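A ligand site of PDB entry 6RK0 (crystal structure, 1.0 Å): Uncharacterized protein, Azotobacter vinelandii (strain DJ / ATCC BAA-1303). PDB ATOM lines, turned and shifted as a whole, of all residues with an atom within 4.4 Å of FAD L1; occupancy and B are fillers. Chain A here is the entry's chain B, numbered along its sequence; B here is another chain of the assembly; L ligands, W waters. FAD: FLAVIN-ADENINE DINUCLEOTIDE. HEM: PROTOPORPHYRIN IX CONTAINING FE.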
ATOM      1  N   ARG A  18     -32.993  16.403 -11.579  1.00  0.00           N
ATOM      2  CA  ARG A  18     -33.113  14.950 -11.523  1.00  0.00           C
ATOM      3  C   ARG A  18     -32.913  14.283 -12.872  1.00  0.00           C
ATOM      4  O   ARG A  18     -32.779  13.066 -12.903  1.00  0.00           O
ATOM      5  CB  ARG A  18     -34.419  14.513 -10.865  1.00  0.00           C
ATOM      6  CG  ARG A  18     -35.635  14.829 -11.633  1.00  0.00           C
ATOM      7  CD  ARG A  18     -36.854  14.370 -10.856  1.00  0.00           C
ATOM      8  NE  ARG A  18     -38.025  14.600 -11.657  1.00  0.00           N
ATOM      9  CZ  ARG A  18     -39.269  14.343 -11.263  1.00  0.00           C
ATOM     10  NH1 ARG A  18     -39.533  13.740 -10.105  1.00  0.00           N
ATOM     11  NH2 ARG A  18     -40.258  14.635 -12.114  1.00  0.00           N
ATOM     12  N   THR A  19     -32.818  15.059 -13.960  1.00  0.00           N
ATOM     13  CA  THR A  19     -32.474  14.541 -15.282  1.00  0.00           C
ATOM     14  C   THR A  19     -31.054  14.890 -15.725  1.00  0.00           C
ATOM     15  O   THR A  19     -30.687  14.665 -16.877  1.00  0.00           O
ATOM     16  CB  THR A  19     -33.475  14.969 -16.370  1.00  0.00           C
ATOM     17  OG1 THR A  19     -33.660  16.399 -16.411  1.00  0.00           O
ATOM     18  CG2 THR A  19     -34.814  14.260 -16.200  1.00  0.00           C
ATOM     19  N   HIS A  20     -30.260  15.438 -14.825  1.00  0.00           N
ATOM     20  CA  HIS A  20     -28.884  15.792 -15.187  1.00  0.00           C
ATOM     21  C   HIS A  20     -28.012  14.527 -15.184  1.00  0.00           C
ATOM     22  O   HIS A  20     -27.797  13.901 -14.136  1.00  0.00           O
ATOM     23  CB  HIS A  20     -28.389  16.835 -14.199  1.00  0.00           C
ATOM     24  CG  HIS A  20     -26.948  17.190 -14.379  1.00  0.00           C
ATOM     25  ND1 HIS A  20     -26.440  17.772 -15.528  1.00  0.00           N
ATOM     26  CD2 HIS A  20     -25.895  16.957 -13.573  1.00  0.00           C
ATOM     27  CE1 HIS A  20     -25.140  17.943 -15.383  1.00  0.00           C
ATOM     28  NE2 HIS A  20     -24.785  17.449 -14.210  1.00  0.00           N
ATOM     29  N   VAL A  21     -27.537  14.172 -16.371  1.00  0.00           N
ATOM     30  CA  VAL A  21     -26.669  13.010 -16.531  1.00  0.00           C
ATOM     31  C   VAL A  21     -25.342  13.306 -15.857  1.00  0.00           C
ATOM     32  O   VAL A  21     -24.674  14.305 -16.165  1.00  0.00           O
ATOM     33  CB  VAL A  21     -26.457  12.722 -18.031  1.00  0.00           C
ATOM     34  CG1 VAL A  21     -25.453  11.593 -18.251  1.00  0.00           C
ATOM     35  CG2 VAL A  21     -27.768  12.414 -18.719  1.00  0.00           C
ATOM     36  N   LYS A  22     -24.935  12.405 -14.967  1.00  0.00           N
ATOM     37  CA  LYS A  22     -23.673  12.529 -14.244  1.00  0.00           C
ATOM     38  C   LYS A  22     -22.623  11.567 -14.774  1.00  0.00           C
ATOM     39  O   LYS A  22     -21.559  11.992 -15.241  1.00  0.00           O
ATOM     40  CB  LYS A  22     -23.923  12.312 -12.757  1.00  0.00           C
ATOM     41  CG  LYS A  22     -24.790  13.472 -12.146  1.00  0.00           C
ATOM     42  CD  LYS A  22     -25.263  13.113 -10.786  1.00  0.00           C
ATOM     43  CE  LYS A  22     -25.378  11.694 -10.886  1.00  0.00           C
ATOM     44  NZ  LYS A  22     -26.289  11.250  -9.863  1.00  0.00           N
ATOM     45  N   ARG A  23     -22.889  10.264 -14.755  1.00  0.00           N
ATOM     46  CA  ARG A  23     -21.909   9.308 -15.266  1.00  0.00           C
ATOM     47  C   ARG A  23     -21.816   9.405 -16.789  1.00  0.00           C
ATOM     48  O   ARG A  23     -22.824   9.506 -17.477  1.00  0.00           O
ATOM     49  CB  ARG A  23     -22.277   7.870 -14.865  1.00  0.00           C
ATOM     50  CG  ARG A  23     -22.602   7.690 -13.399  1.00  0.00           C
ATOM     51  CD  ARG A  23     -22.221   6.292 -12.947  1.00  0.00           C
ATOM     52  NE  ARG A  23     -20.781   6.230 -12.846  1.00  0.00           N
ATOM     53  CZ  ARG A  23     -20.093   6.616 -11.796  1.00  0.00           C
ATOM     54  NH1 ARG A  23     -18.788   6.656 -11.846  1.00  0.00           N
ATOM     55  NH2 ARG A  23     -20.744   7.031 -10.700  1.00  0.00           N
ATOM     56  N   SER A  93     -34.946   2.459 -24.968  1.00  0.00           N
ATOM     57  CA  SER A  93     -33.562   2.106 -25.295  1.00  0.00           C
ATOM     58  C   SER A  93     -33.481   1.385 -26.638  1.00  0.00           C
ATOM     59  O   SER A  93     -34.363   0.600 -26.990  1.00  0.00           O
ATOM     60  CB  SER A  93     -32.936   1.250 -24.205  1.00  0.00           C
ATOM     61  OG  SER A  93     -33.653   0.011 -24.087  1.00  0.00           O
ATOM     62  N   LEU A  95     -30.335  -0.785 -28.552  1.00  0.00           N
ATOM     63  CA  LEU A  95     -28.994  -1.358 -28.578  1.00  0.00           C
ATOM     64  C   LEU A  95     -28.494  -1.367 -30.012  1.00  0.00           C
ATOM     65  O   LEU A  95     -29.088  -1.991 -30.896  1.00  0.00           O
ATOM     66  CB  LEU A  95     -29.030  -2.762 -27.992  1.00  0.00           C
ATOM     67  CG  LEU A  95     -27.736  -3.554 -28.040  1.00  0.00           C
ATOM     68  CD1 LEU A  95     -26.570  -2.843 -27.334  1.00  0.00           C
ATOM     69  CD2 LEU A  95     -28.015  -4.946 -27.459  1.00  0.00           C
ATOM     70  N   CYS A 109     -21.106  -0.594 -25.262  1.00  0.00           N
ATOM     71  CA  CYS A 109     -22.053  -0.799 -26.337  1.00  0.00           C
ATOM     72  C   CYS A 109     -22.393   0.546 -26.936  1.00  0.00           C
ATOM     73  O   CYS A 109     -22.353   1.578 -26.274  1.00  0.00           O
ATOM     74  CB  CYS A 109     -23.293  -1.569 -25.876  1.00  0.00           C
ATOM     75  SG  CYS A 109     -24.473  -0.556 -24.917  1.00  0.00           S
ATOM     76  N   PHE A 111     -25.452   2.736 -28.502  1.00  0.00           N
ATOM     77  CA  PHE A 111     -26.851   2.739 -28.073  1.00  0.00           C
ATOM     78  C   PHE A 111     -27.403   4.133 -28.214  1.00  0.00           C
ATOM     79  O   PHE A 111     -26.669   5.123 -28.338  1.00  0.00           O
ATOM     80  CB  PHE A 111     -26.982   2.270 -26.612  1.00  0.00           C
ATOM     81  CG  PHE A 111     -26.305   3.189 -25.625  1.00  0.00           C
ATOM     82  CD1 PHE A 111     -26.981   4.291 -25.090  1.00  0.00           C
ATOM     83  CD2 PHE A 111     -24.989   2.985 -25.244  1.00  0.00           C
ATOM     84  CE1 PHE A 111     -26.380   5.146 -24.199  1.00  0.00           C
ATOM     85  CE2 PHE A 111     -24.380   3.886 -24.340  1.00  0.00           C
ATOM     86  CZ  PHE A 111     -25.081   4.963 -23.850  1.00  0.00           C
ATOM     87  N   SER A 113     -30.537   6.029 -25.820  1.00  0.00           N
ATOM     88  CA  SER A 113     -31.585   5.895 -24.821  1.00  0.00           C
ATOM     89  C   SER A 113     -32.084   7.247 -24.368  1.00  0.00           C
ATOM     90  O   SER A 113     -31.350   8.233 -24.341  1.00  0.00           O
ATOM     91  CB  SER A 113     -31.161   5.037 -23.645  1.00  0.00           C
ATOM     92  OG  SER A 113     -30.026   5.578 -22.977  1.00  0.00           O
ATOM     93  N   VAL A 114     -33.361   7.257 -23.966  1.00  0.00           N
ATOM     94  CA  VAL A 114     -34.018   8.441 -23.442  1.00  0.00           C
ATOM     95  C   VAL A 114     -34.839   8.033 -22.237  1.00  0.00           C
ATOM     96  O   VAL A 114     -35.480   6.960 -22.237  1.00  0.00           O
ATOM     97  CB  VAL A 114     -34.822   9.207 -24.517  1.00  0.00           C
ATOM     98  CG1 VAL A 114     -35.889   8.319 -25.154  1.00  0.00           C
ATOM     99  CG2 VAL A 114     -35.389  10.544 -23.965  1.00  0.00           C
ATOM    100  N   MET A 115     -34.788   8.848 -21.204  1.00  0.00           N
ATOM    101  CA  MET A 115     -35.654   8.727 -20.032  1.00  0.00           C
ATOM    102  C   MET A 115     -36.523   9.961 -19.952  1.00  0.00           C
ATOM    103  O   MET A 115     -36.005  11.090 -20.003  1.00  0.00           O
ATOM    104  CB  MET A 115     -34.859   8.593 -18.751  1.00  0.00           C
ATOM    105  CG  MET A 115     -34.035   7.309 -18.675  1.00  0.00           C
ATOM    106  SD  MET A 115     -33.114   7.200 -17.145  1.00  0.00           S
ATOM    107  CE  MET A 115     -32.210   5.700 -17.393  1.00  0.00           C
ATOM    108  N   SER A 170     -33.903  13.175 -20.509  1.00  0.00           N
ATOM    109  CA  SER A 170     -32.467  13.070 -20.701  1.00  0.00           C
ATOM    110  C   SER A 170     -32.201  11.971 -21.732  1.00  0.00           C
ATOM    111  O   SER A 170     -32.869  10.918 -21.724  1.00  0.00           O
ATOM    112  CB  SER A 170     -31.778  12.723 -19.388  1.00  0.00           C
ATOM    113  OG  SER A 170     -32.313  11.560 -18.766  1.00  0.00           O
ATOM    114  N   CYS A 171     -31.218  12.193 -22.599  1.00  0.00           N
ATOM    115  CA  CYS A 171     -30.745  11.152 -23.502  1.00  0.00           C
ATOM    116  C   CYS A 171     -29.286  10.862 -23.239  1.00  0.00           C
ATOM    117  O   CYS A 171     -28.511  11.741 -22.833  1.00  0.00           O
ATOM    118  CB  CYS A 171     -30.858  11.580 -24.968  1.00  0.00           C
ATOM    119  SG  CYS A 171     -32.421  12.265 -25.466  1.00  0.00           S
ATOM    120  N   LYS A 172     -28.880   9.638 -23.556  1.00  0.00           N
ATOM    121  CA  LYS A 172     -27.480   9.287 -23.717  1.00  0.00           C
ATOM    122  C   LYS A 172     -27.370   8.544 -25.035  1.00  0.00           C
ATOM    123  O   LYS A 172     -28.216   7.707 -25.365  1.00  0.00           O
ATOM    124  CB  LYS A 172     -26.933   8.426 -22.566  1.00  0.00           C
ATOM    125  CG  LYS A 172     -26.784   9.156 -21.258  1.00  0.00           C
ATOM    126  CD  LYS A 172     -26.425   8.248 -20.082  1.00  0.00           C
ATOM    127  CE  LYS A 172     -24.929   7.771 -20.089  1.00  0.00           C
ATOM    128  NZ  LYS A 172     -24.736   6.844 -18.909  1.00  0.00           N
ATOM    129  N   LEU B  44     -29.876  -7.787 -22.793  1.00  0.00           N
ATOM    130  CA  LEU B  44     -30.384  -6.472 -22.400  1.00  0.00           C
ATOM    131  C   LEU B  44     -31.558  -6.566 -21.428  1.00  0.00           C
ATOM    132  O   LEU B  44     -32.633  -7.096 -21.790  1.00  0.00           O
ATOM    133  CB  LEU B  44     -30.801  -5.670 -23.636  1.00  0.00           C
ATOM    134  CG  LEU B  44     -31.386  -4.287 -23.389  1.00  0.00           C
ATOM    135  CD1 LEU B  44     -30.415  -3.383 -22.647  1.00  0.00           C
ATOM    136  CD2 LEU B  44     -31.862  -3.641 -24.686  1.00  0.00           C
ATOM    137  N   PHE B  56     -36.988   4.776 -11.307  1.00  0.00           N
ATOM    138  CA  PHE B  56     -36.192   4.800 -12.503  1.00  0.00           C
ATOM    139  C   PHE B  56     -36.098   3.443 -13.160  1.00  0.00           C
ATOM    140  O   PHE B  56     -36.065   2.398 -12.498  1.00  0.00           O
ATOM    141  CB  PHE B  56     -34.768   5.269 -12.176  1.00  0.00           C
ATOM    142  CG  PHE B  56     -34.645   6.771 -12.123  1.00  0.00           C
ATOM    143  CD1 PHE B  56     -34.496   7.493 -13.290  1.00  0.00           C
ATOM    144  CD2 PHE B  56     -34.650   7.466 -10.922  1.00  0.00           C
ATOM    145  CE1 PHE B  56     -34.410   8.874 -13.287  1.00  0.00           C
ATOM    146  CE2 PHE B  56     -34.546   8.833 -10.900  1.00  0.00           C
ATOM    147  CZ  PHE B  56     -34.417   9.561 -12.074  1.00  0.00           C
ATOM    148  N   THR B  58     -33.484   1.584 -15.568  1.00  0.00           N
ATOM    149  CA  THR B  58     -32.118   1.668 -16.090  1.00  0.00           C
ATOM    150  C   THR B  58     -31.863   0.541 -17.065  1.00  0.00           C
ATOM    151  O   THR B  58     -31.886  -0.632 -16.642  1.00  0.00           O
ATOM    152  CB  THR B  58     -31.121   1.617 -14.944  1.00  0.00           C
ATOM    153  OG1 THR B  58     -31.348   2.707 -14.048  1.00  0.00           O
ATOM    154  CG2 THR B  58     -29.679   1.681 -15.459  1.00  0.00           C
ATOM    155  N   PRO B  59     -31.568   0.818 -18.337  1.00  0.00           N
ATOM    156  CA  PRO B  59     -31.141  -0.252 -19.248  1.00  0.00           C
ATOM    157  C   PRO B  59     -29.753  -0.719 -18.874  1.00  0.00           C
ATOM    158  O   PRO B  59     -28.880   0.108 -18.555  1.00  0.00           O
ATOM    159  CB  PRO B  59     -31.136   0.422 -20.621  1.00  0.00           C
ATOM    160  CG  PRO B  59     -31.386   1.842 -20.425  1.00  0.00           C
ATOM    161  CD  PRO B  59     -31.600   2.141 -19.003  1.00  0.00           C
ATOM    162  N   THR B  60     -29.525  -2.039 -18.906  1.00  0.00           N
ATOM    163  CA  THR B  60     -28.205  -2.544 -18.568  1.00  0.00           C
ATOM    164  C   THR B  60     -28.026  -3.929 -19.170  1.00  0.00           C
ATOM    165  O   THR B  60     -28.994  -4.663 -19.401  1.00  0.00           O
ATOM    166  CB  THR B  60     -28.040  -2.548 -17.046  1.00  0.00           C
ATOM    167  OG1 THR B  60     -26.666  -2.776 -16.748  1.00  0.00           O
ATOM    168  CG2 THR B  60     -28.954  -3.595 -16.357  1.00  0.00           C
ATOM    169  N   PHE B  61     -26.776  -4.328 -19.327  1.00  0.00           N
ATOM    170  CA  PHE B  61     -26.520  -5.714 -19.679  1.00  0.00           C
ATOM    171  C   PHE B  61     -26.637  -6.617 -18.464  1.00  0.00           C
ATOM    172  O   PHE B  61     -26.505  -6.178 -17.314  1.00  0.00           O
ATOM    173  CB  PHE B  61     -25.160  -5.859 -20.325  1.00  0.00           C
ATOM    174  CG  PHE B  61     -25.115  -5.250 -21.683  1.00  0.00           C
ATOM    175  CD1 PHE B  61     -24.287  -4.211 -21.949  1.00  0.00           C
ATOM    176  CD2 PHE B  61     -26.074  -5.590 -22.627  1.00  0.00           C
ATOM    177  CE1 PHE B  61     -24.238  -3.634 -23.191  1.00  0.00           C
ATOM    178  CE2 PHE B  61     -26.076  -4.983 -23.892  1.00  0.00           C
ATOM    179  CZ  PHE B  61     -25.124  -4.000 -24.148  1.00  0.00           C
ATOM    180  N   HIS B  72     -23.390  -5.197 -13.885  1.00  0.00           N
ATOM    181  CA  HIS B  72     -22.209  -4.483 -13.421  1.00  0.00           C
ATOM    182  C   HIS B  72     -22.341  -2.990 -13.695  1.00  0.00           C
ATOM    183  O   HIS B  72     -23.113  -2.550 -14.551  1.00  0.00           O
ATOM    184  CB  HIS B  72     -20.917  -5.007 -14.095  1.00  0.00           C
ATOM    185  CG  HIS B  72     -20.634  -4.352 -15.429  1.00  0.00           C
ATOM    186  ND1 HIS B  72     -21.448  -4.479 -16.542  1.00  0.00           N
ATOM    187  CD2 HIS B  72     -19.644  -3.508 -15.804  1.00  0.00           C
ATOM    188  CE1 HIS B  72     -20.969  -3.731 -17.512  1.00  0.00           C
ATOM    189  NE2 HIS B  72     -19.875  -3.145 -17.102  1.00  0.00           N
ATOM    190  N   GLY B  73     -21.511  -2.210 -13.004  1.00  0.00           N
ATOM    191  CA  GLY B  73     -21.429  -0.777 -13.250  1.00  0.00           C
ATOM    192  C   GLY B  73     -20.399  -0.192 -12.314  1.00  0.00           C
ATOM    193  O   GLY B  73     -19.457  -0.868 -11.900  1.00  0.00           O
ATOM    194  N   ARG B  78     -25.139   5.042  -8.262  1.00  0.00           N
ATOM    195  CA  ARG B  78     -26.310   5.176  -7.380  1.00  0.00           C
ATOM    196  C   ARG B  78     -27.155   3.909  -7.351  1.00  0.00           C
ATOM    197  O   ARG B  78     -27.773   3.619  -6.310  1.00  0.00           O
ATOM    198  CB  ARG B  78     -27.150   6.399  -7.771  1.00  0.00           C
ATOM    199  CG  ARG B  78     -27.786   6.323  -9.138  1.00  0.00           C
ATOM    200  CD  ARG B  78     -28.755   7.478  -9.287  1.00  0.00           C
ATOM    201  NE  ARG B  78     -29.466   7.402 -10.539  1.00  0.00           N
ATOM    202  CZ  ARG B  78     -30.489   8.187 -10.810  1.00  0.00           C
ATOM    203  NH1 ARG B  78     -30.909   9.112  -9.941  1.00  0.00           N
ATOM    204  NH2 ARG B  78     -31.143   8.041 -11.953  1.00  0.00           N
HETATM  205  PA  FAD L   1     -26.628   9.034 -13.284  1.00  0.00           P
HETATM  206  O1A FAD L   1     -25.760   9.796 -14.217  1.00  0.00           O
HETATM  207  O2A FAD L   1     -26.327   9.090 -11.839  1.00  0.00           O
HETATM  208  O5B FAD L   1     -28.153   9.415 -13.523  1.00  0.00           O
HETATM  209  C5B FAD L   1     -28.564  10.797 -13.445  1.00  0.00           C
HETATM  210  C4B FAD L   1     -29.587  11.066 -14.495  1.00  0.00           C
HETATM  211  O4B FAD L   1     -29.034  10.823 -15.809  1.00  0.00           O
HETATM  212  C3B FAD L   1     -30.810  10.153 -14.448  1.00  0.00           C
HETATM  213  O3B FAD L   1     -31.743  10.522 -13.444  1.00  0.00           O
HETATM  214  C2B FAD L   1     -31.338  10.280 -15.888  1.00  0.00           C
HETATM  215  O2B FAD L   1     -32.108  11.465 -16.012  1.00  0.00           O
HETATM  216  C1B FAD L   1     -30.046  10.407 -16.700  1.00  0.00           C
HETATM  217  N9A FAD L   1     -29.636   9.124 -17.292  1.00  0.00           N
HETATM  218  C8A FAD L   1     -28.893   8.143 -16.717  1.00  0.00           C
HETATM  219  N7A FAD L   1     -28.735   7.090 -17.471  1.00  0.00           N
HETATM  220  C5A FAD L   1     -29.439   7.401 -18.632  1.00  0.00           C
HETATM  221  C6A FAD L   1     -29.673   6.679 -19.829  1.00  0.00           C
HETATM  222  N6A FAD L   1     -29.224   5.438 -20.064  1.00  0.00           N
HETATM  223  N1A FAD L   1     -30.440   7.275 -20.770  1.00  0.00           N
HETATM  224  C2A FAD L   1     -30.921   8.512 -20.533  1.00  0.00           C
HETATM  225  N3A FAD L   1     -30.759   9.272 -19.442  1.00  0.00           N
HETATM  226  C4A FAD L   1     -30.010   8.654 -18.535  1.00  0.00           C
HETATM  227  N1  FAD L   1     -24.611   0.853 -17.490  1.00  0.00           N
HETATM  228  C2  FAD L   1     -23.851   0.012 -16.735  1.00  0.00           C
HETATM  229  O2  FAD L   1     -23.331   0.389 -15.684  1.00  0.00           O
HETATM  230  N3  FAD L   1     -23.653  -1.287 -17.125  1.00  0.00           N
HETATM  231  C4  FAD L   1     -24.188  -1.853 -18.259  1.00  0.00           C
HETATM  232  O4  FAD L   1     -24.028  -3.049 -18.511  1.00  0.00           O
HETATM  233  C4X FAD L   1     -24.938  -0.939 -19.101  1.00  0.00           C
HETATM  234  N5  FAD L   1     -25.446  -1.401 -20.249  1.00  0.00           N
HETATM  235  C5X FAD L   1     -26.271  -0.540 -20.975  1.00  0.00           C
HETATM  236  C6  FAD L   1     -26.863  -1.011 -22.159  1.00  0.00           C
HETATM  237  C7  FAD L   1     -27.704  -0.190 -22.914  1.00  0.00           C
HETATM  238  C7M FAD L   1     -28.312  -0.716 -24.187  1.00  0.00           C
HETATM  239  C8  FAD L   1     -27.934   1.132 -22.497  1.00  0.00           C
HETATM  240  C8M FAD L   1     -28.857   2.039 -23.244  1.00  0.00           C
HETATM  241  C9  FAD L   1     -27.316   1.610 -21.339  1.00  0.00           C
HETATM  242  C9A FAD L   1     -26.476   0.799 -20.586  1.00  0.00           C
HETATM  243  N10 FAD L   1     -25.826   1.254 -19.413  1.00  0.00           N
HETATM  244  C10 FAD L   1     -25.113   0.394 -18.626  1.00  0.00           C
HETATM  245  C1' FAD L   1     -25.971   2.634 -18.927  1.00  0.00           C
HETATM  246  C2' FAD L   1     -27.072   2.775 -17.885  1.00  0.00           C
HETATM  247  O2' FAD L   1     -28.336   2.816 -18.526  1.00  0.00           O
HETATM  248  C3' FAD L   1     -26.888   4.049 -17.068  1.00  0.00           C
HETATM  249  O3' FAD L   1     -26.876   5.170 -17.945  1.00  0.00           O
HETATM  250  C4' FAD L   1     -25.610   4.071 -16.223  1.00  0.00           C
HETATM  251  O4' FAD L   1     -25.506   2.843 -15.500  1.00  0.00           O
HETATM  252  C5' FAD L   1     -25.570   5.246 -15.280  1.00  0.00           C
HETATM  253  O5' FAD L   1     -26.748   5.202 -14.439  1.00  0.00           O
HETATM  254  P   FAD L   1     -26.824   6.087 -13.151  1.00  0.00           P
HETATM  255  O1P FAD L   1     -25.681   5.803 -12.219  1.00  0.00           O
HETATM  256  O2P FAD L   1     -28.227   5.941 -12.606  1.00  0.00           O
HETATM  257  O3P FAD L   1     -26.656   7.544 -13.792  1.00  0.00           O
HETATM  258  CHA HEM L   2     -19.932   0.897 -17.261  1.00  0.00           C
HETATM  259  CHB HEM L   2     -20.781  -2.124 -20.879  1.00  0.00           C
HETATM  260  CHC HEM L   2     -17.402  -5.094 -19.141  1.00  0.00           C
HETATM  261  CHD HEM L   2     -16.360  -1.930 -15.705  1.00  0.00           C
HETATM  262  C1A HEM L   2     -20.432   0.323 -18.403  1.00  0.00           C
HETATM  263  C2A HEM L   2     -21.469   0.939 -19.221  1.00  0.00           C
HETATM  264  C3A HEM L   2     -21.720   0.094 -20.237  1.00  0.00           C
HETATM  265  C4A HEM L   2     -20.832  -1.038 -20.043  1.00  0.00           C
HETATM  266  CMA HEM L   2     -22.680   0.241 -21.391  1.00  0.00           C
HETATM  267  CAA HEM L   2     -22.114   2.313 -18.980  1.00  0.00           C
HETATM  268  CBA HEM L   2     -21.239   3.497 -19.475  1.00  0.00           C
HETATM  269  CGA HEM L   2     -22.146   4.686 -19.644  1.00  0.00           C
HETATM  270  O1A HEM L   2     -22.501   5.101 -20.800  1.00  0.00           O
HETATM  271  O2A HEM L   2     -22.574   5.263 -18.586  1.00  0.00           O
HETATM  272  C1B HEM L   2     -19.929  -3.184 -20.755  1.00  0.00           C
HETATM  273  C2B HEM L   2     -19.934  -4.352 -21.602  1.00  0.00           C
HETATM  274  C3B HEM L   2     -18.992  -5.171 -21.093  1.00  0.00           C
HETATM  275  C4B HEM L   2     -18.390  -4.540 -19.940  1.00  0.00           C
HETATM  276  CMB HEM L   2     -20.864  -4.524 -22.796  1.00  0.00           C
HETATM  277  CAB HEM L   2     -18.520  -6.537 -21.551  1.00  0.00           C
HETATM  278  CBB HEM L   2     -18.811  -7.104 -22.725  1.00  0.00           C
HETATM  279  C1C HEM L   2     -16.828  -4.494 -18.055  1.00  0.00           C
HETATM  280  C2C HEM L   2     -15.776  -5.075 -17.272  1.00  0.00           C
HETATM  281  C3C HEM L   2     -15.437  -4.170 -16.348  1.00  0.00           C
HETATM  282  C4C HEM L   2     -16.312  -3.040 -16.515  1.00  0.00           C
HETATM  283  CMC HEM L   2     -15.236  -6.479 -17.497  1.00  0.00           C
HETATM  284  CAC HEM L   2     -14.375  -4.266 -15.289  1.00  0.00           C
HETATM  285  CBC HEM L   2     -13.193  -4.876 -15.552  1.00  0.00           C
HETATM  286  C1D HEM L   2     -17.271  -0.897 -15.789  1.00  0.00           C
HETATM  287  C2D HEM L   2     -17.343   0.229 -14.904  1.00  0.00           C
HETATM  288  C3D HEM L   2     -18.334   1.013 -15.325  1.00  0.00           C
HETATM  289  C4D HEM L   2     -18.908   0.380 -16.500  1.00  0.00           C
HETATM  290  CMD HEM L   2     -16.428   0.465 -13.696  1.00  0.00           C
HETATM  291  CAD HEM L   2     -18.757   2.367 -14.773  1.00  0.00           C
HETATM  292  CBD HEM L   2     -18.033   3.501 -15.520  1.00  0.00           C
HETATM  293  CGD HEM L   2     -18.276   4.835 -14.842  1.00  0.00           C
HETATM  294  O1D HEM L   2     -19.310   5.488 -15.098  1.00  0.00           O
HETATM  295  O2D HEM L   2     -17.438   5.248 -14.006  1.00  0.00           O
HETATM  296  NA  HEM L   2     -20.046  -0.882 -18.923  1.00  0.00           N
HETATM  297  NB  HEM L   2     -18.995  -3.300 -19.755  1.00  0.00           N
HETATM  298  NC  HEM L   2     -17.133  -3.259 -17.579  1.00  0.00           N
HETATM  299  ND  HEM L   2     -18.232  -0.789 -16.763  1.00  0.00           N
HETATM  300 FE   HEM L   2     -18.603  -2.079 -18.216  1.00  0.00          FE
HETATM  301  O   HOH W   1     -25.250   8.561 -16.738  1.00  0.00           O
HETATM  302  O   HOH W   2     -30.600   6.090 -14.033  1.00  0.00           O
HETATM  303  O   HOH W   3     -24.145  -5.042 -16.636  1.00  0.00           O
HETATM  304  O   HOH W   4     -25.565   3.382 -10.961  1.00  0.00           O
HETATM  305  O   HOH W   5     -25.396   4.921 -21.049  1.00  0.00           O
HETATM  306  O   HOH W   6     -29.148   3.312 -12.516  1.00  0.00           O
HETATM  307  O   HOH W   7     -22.470   2.615 -14.540  1.00  0.00           O
HETATM  308  O   HOH W   8     -26.739   1.992 -13.133  1.00  0.00           O
HETATM  309  O   HOH W   9     -32.142  11.777 -10.356  1.00  0.00           O
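Residues that only touch FAD L1: Thr 19, His 20, Val 21, Cys 109, Phe 111, Met 115, Cys 171, Leu 44 of chain B, Phe 56 of chain B, Thr 58 of chain B and Gly 73 of chain B.
Hydrophobic or aromatic side chains that line FAD L1: Val 21, Phe 111, Met 115, Leu 44 of chain B, Phe 56 of chain B, Pro 59 of chain B, Phe 61 of chain B and His 72 of chain B.
Of the 25 residues printed, 22 come within 4 Å of FAD L1.
O of Ser 170 is in hydrogen-bond range of N of Met 115 (2.9 Å).
The backbone NH of Ser 113 sits at hydrogen-bond distance from the backbone carbonyl oxygen of Lys 172.
Water W4 bridges an oxygen (O1P) of FAD L1 (2.7 Å) and the backbone NH of Arg 78 of chain B (3.2 Å).
Water W2 lies within hydrogen-bond range of O2P of FAD L1, NH2 of Arg 78 of chain B and OG1 of Thr 58 of chain B.
Water W6 lies within hydrogen-bond range of the side-chain hydroxyl (OG1) of Thr 58 of chain B (2.7 Å) and an oxygen (O2P) of FAD L1 (2.8 Å).
Water W1 lies within hydrogen-bond range of O of Arg 23 (2.7 Å), NZ of Lys 172 (2.8 Å) and O1A of FAD L1 (2.9 Å).
Water W5 lies within hydrogen-bond range of an oxygen (O1A) of HEM L2, the side-chain amino group of Lys 172 and an oxygen (O3') of FAD L1.
Water W9 lies within hydrogen-bond range of the backbone carbonyl oxygen (O) of Arg 18 (2.9 Å), the guanidinium group (NH1) of Arg 78 of chain B (3.0 Å) and an oxygen (O3B) of FAD L1 (3.4 Å).
O2' of FAD L1 lies within hydrogen-bond range of O of Pro 59 of chain B (2.8 Å).
The side-chain hydroxyl (OG) of Ser 170 sits at hydrogen-bond distance from an oxygen (O2B) of FAD L1, 2.8 Å away.
O3B of FAD L1 is in hydrogen-bond range of O of Arg 18 (2.8 Å).
A nitrogen (N1A) of FAD L1 sits at hydrogen-bond distance from the side-chain hydroxyl (OG) of Ser 113 (2.8 Å).
The guanidinium group (NE) of Arg 78 of chain B is in salt-bridge range of an oxygen (O2P) of FAD L1 (2.8 Å).
O1A of FAD L1 lies within hydrogen-bond range of N of Lys 22.
An oxygen (O2A) of FAD L1 lies within salt-bridge range of the side-chain amino group (NZ) of Lys 22, at 2.9 Å.
An oxygen (O3') of FAD L1 lies within hydrogen-bond range of the side-chain amino group (NZ) of Lys 172 (2.9 Å).
The backbone carbonyl oxygen (O) of His 72 of chain B lies within hydrogen-bond range of a nitrogen (N3) of FAD L1 (2.9 Å).
O1A of FAD L1 is in hydrogen-bond range of N of Arg 23 (3.0 Å).
The side-chain hydroxyl (OG1) of Thr 60 of chain B sits close to an oxygen (O4) of FAD L1 (3.2 Å).
The backbone NH (N) of Phe 61 of chain B is in hydrogen-bond range of an oxygen (O4) of FAD L1.
The side-chain amino group (NZ) of Lys 172 lies within salt-bridge range of an oxygen (O2A) of HEM L2, at 2.7 Å.
An iron atom (FE) of HEM L2 is bound by a ring nitrogen (NE2) of His 72 of chain B (2.0 Å).
The guanidinium group of Arg 23 is in salt-bridge range of an oxygen (O1D) of HEM L2 (2.8 Å).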
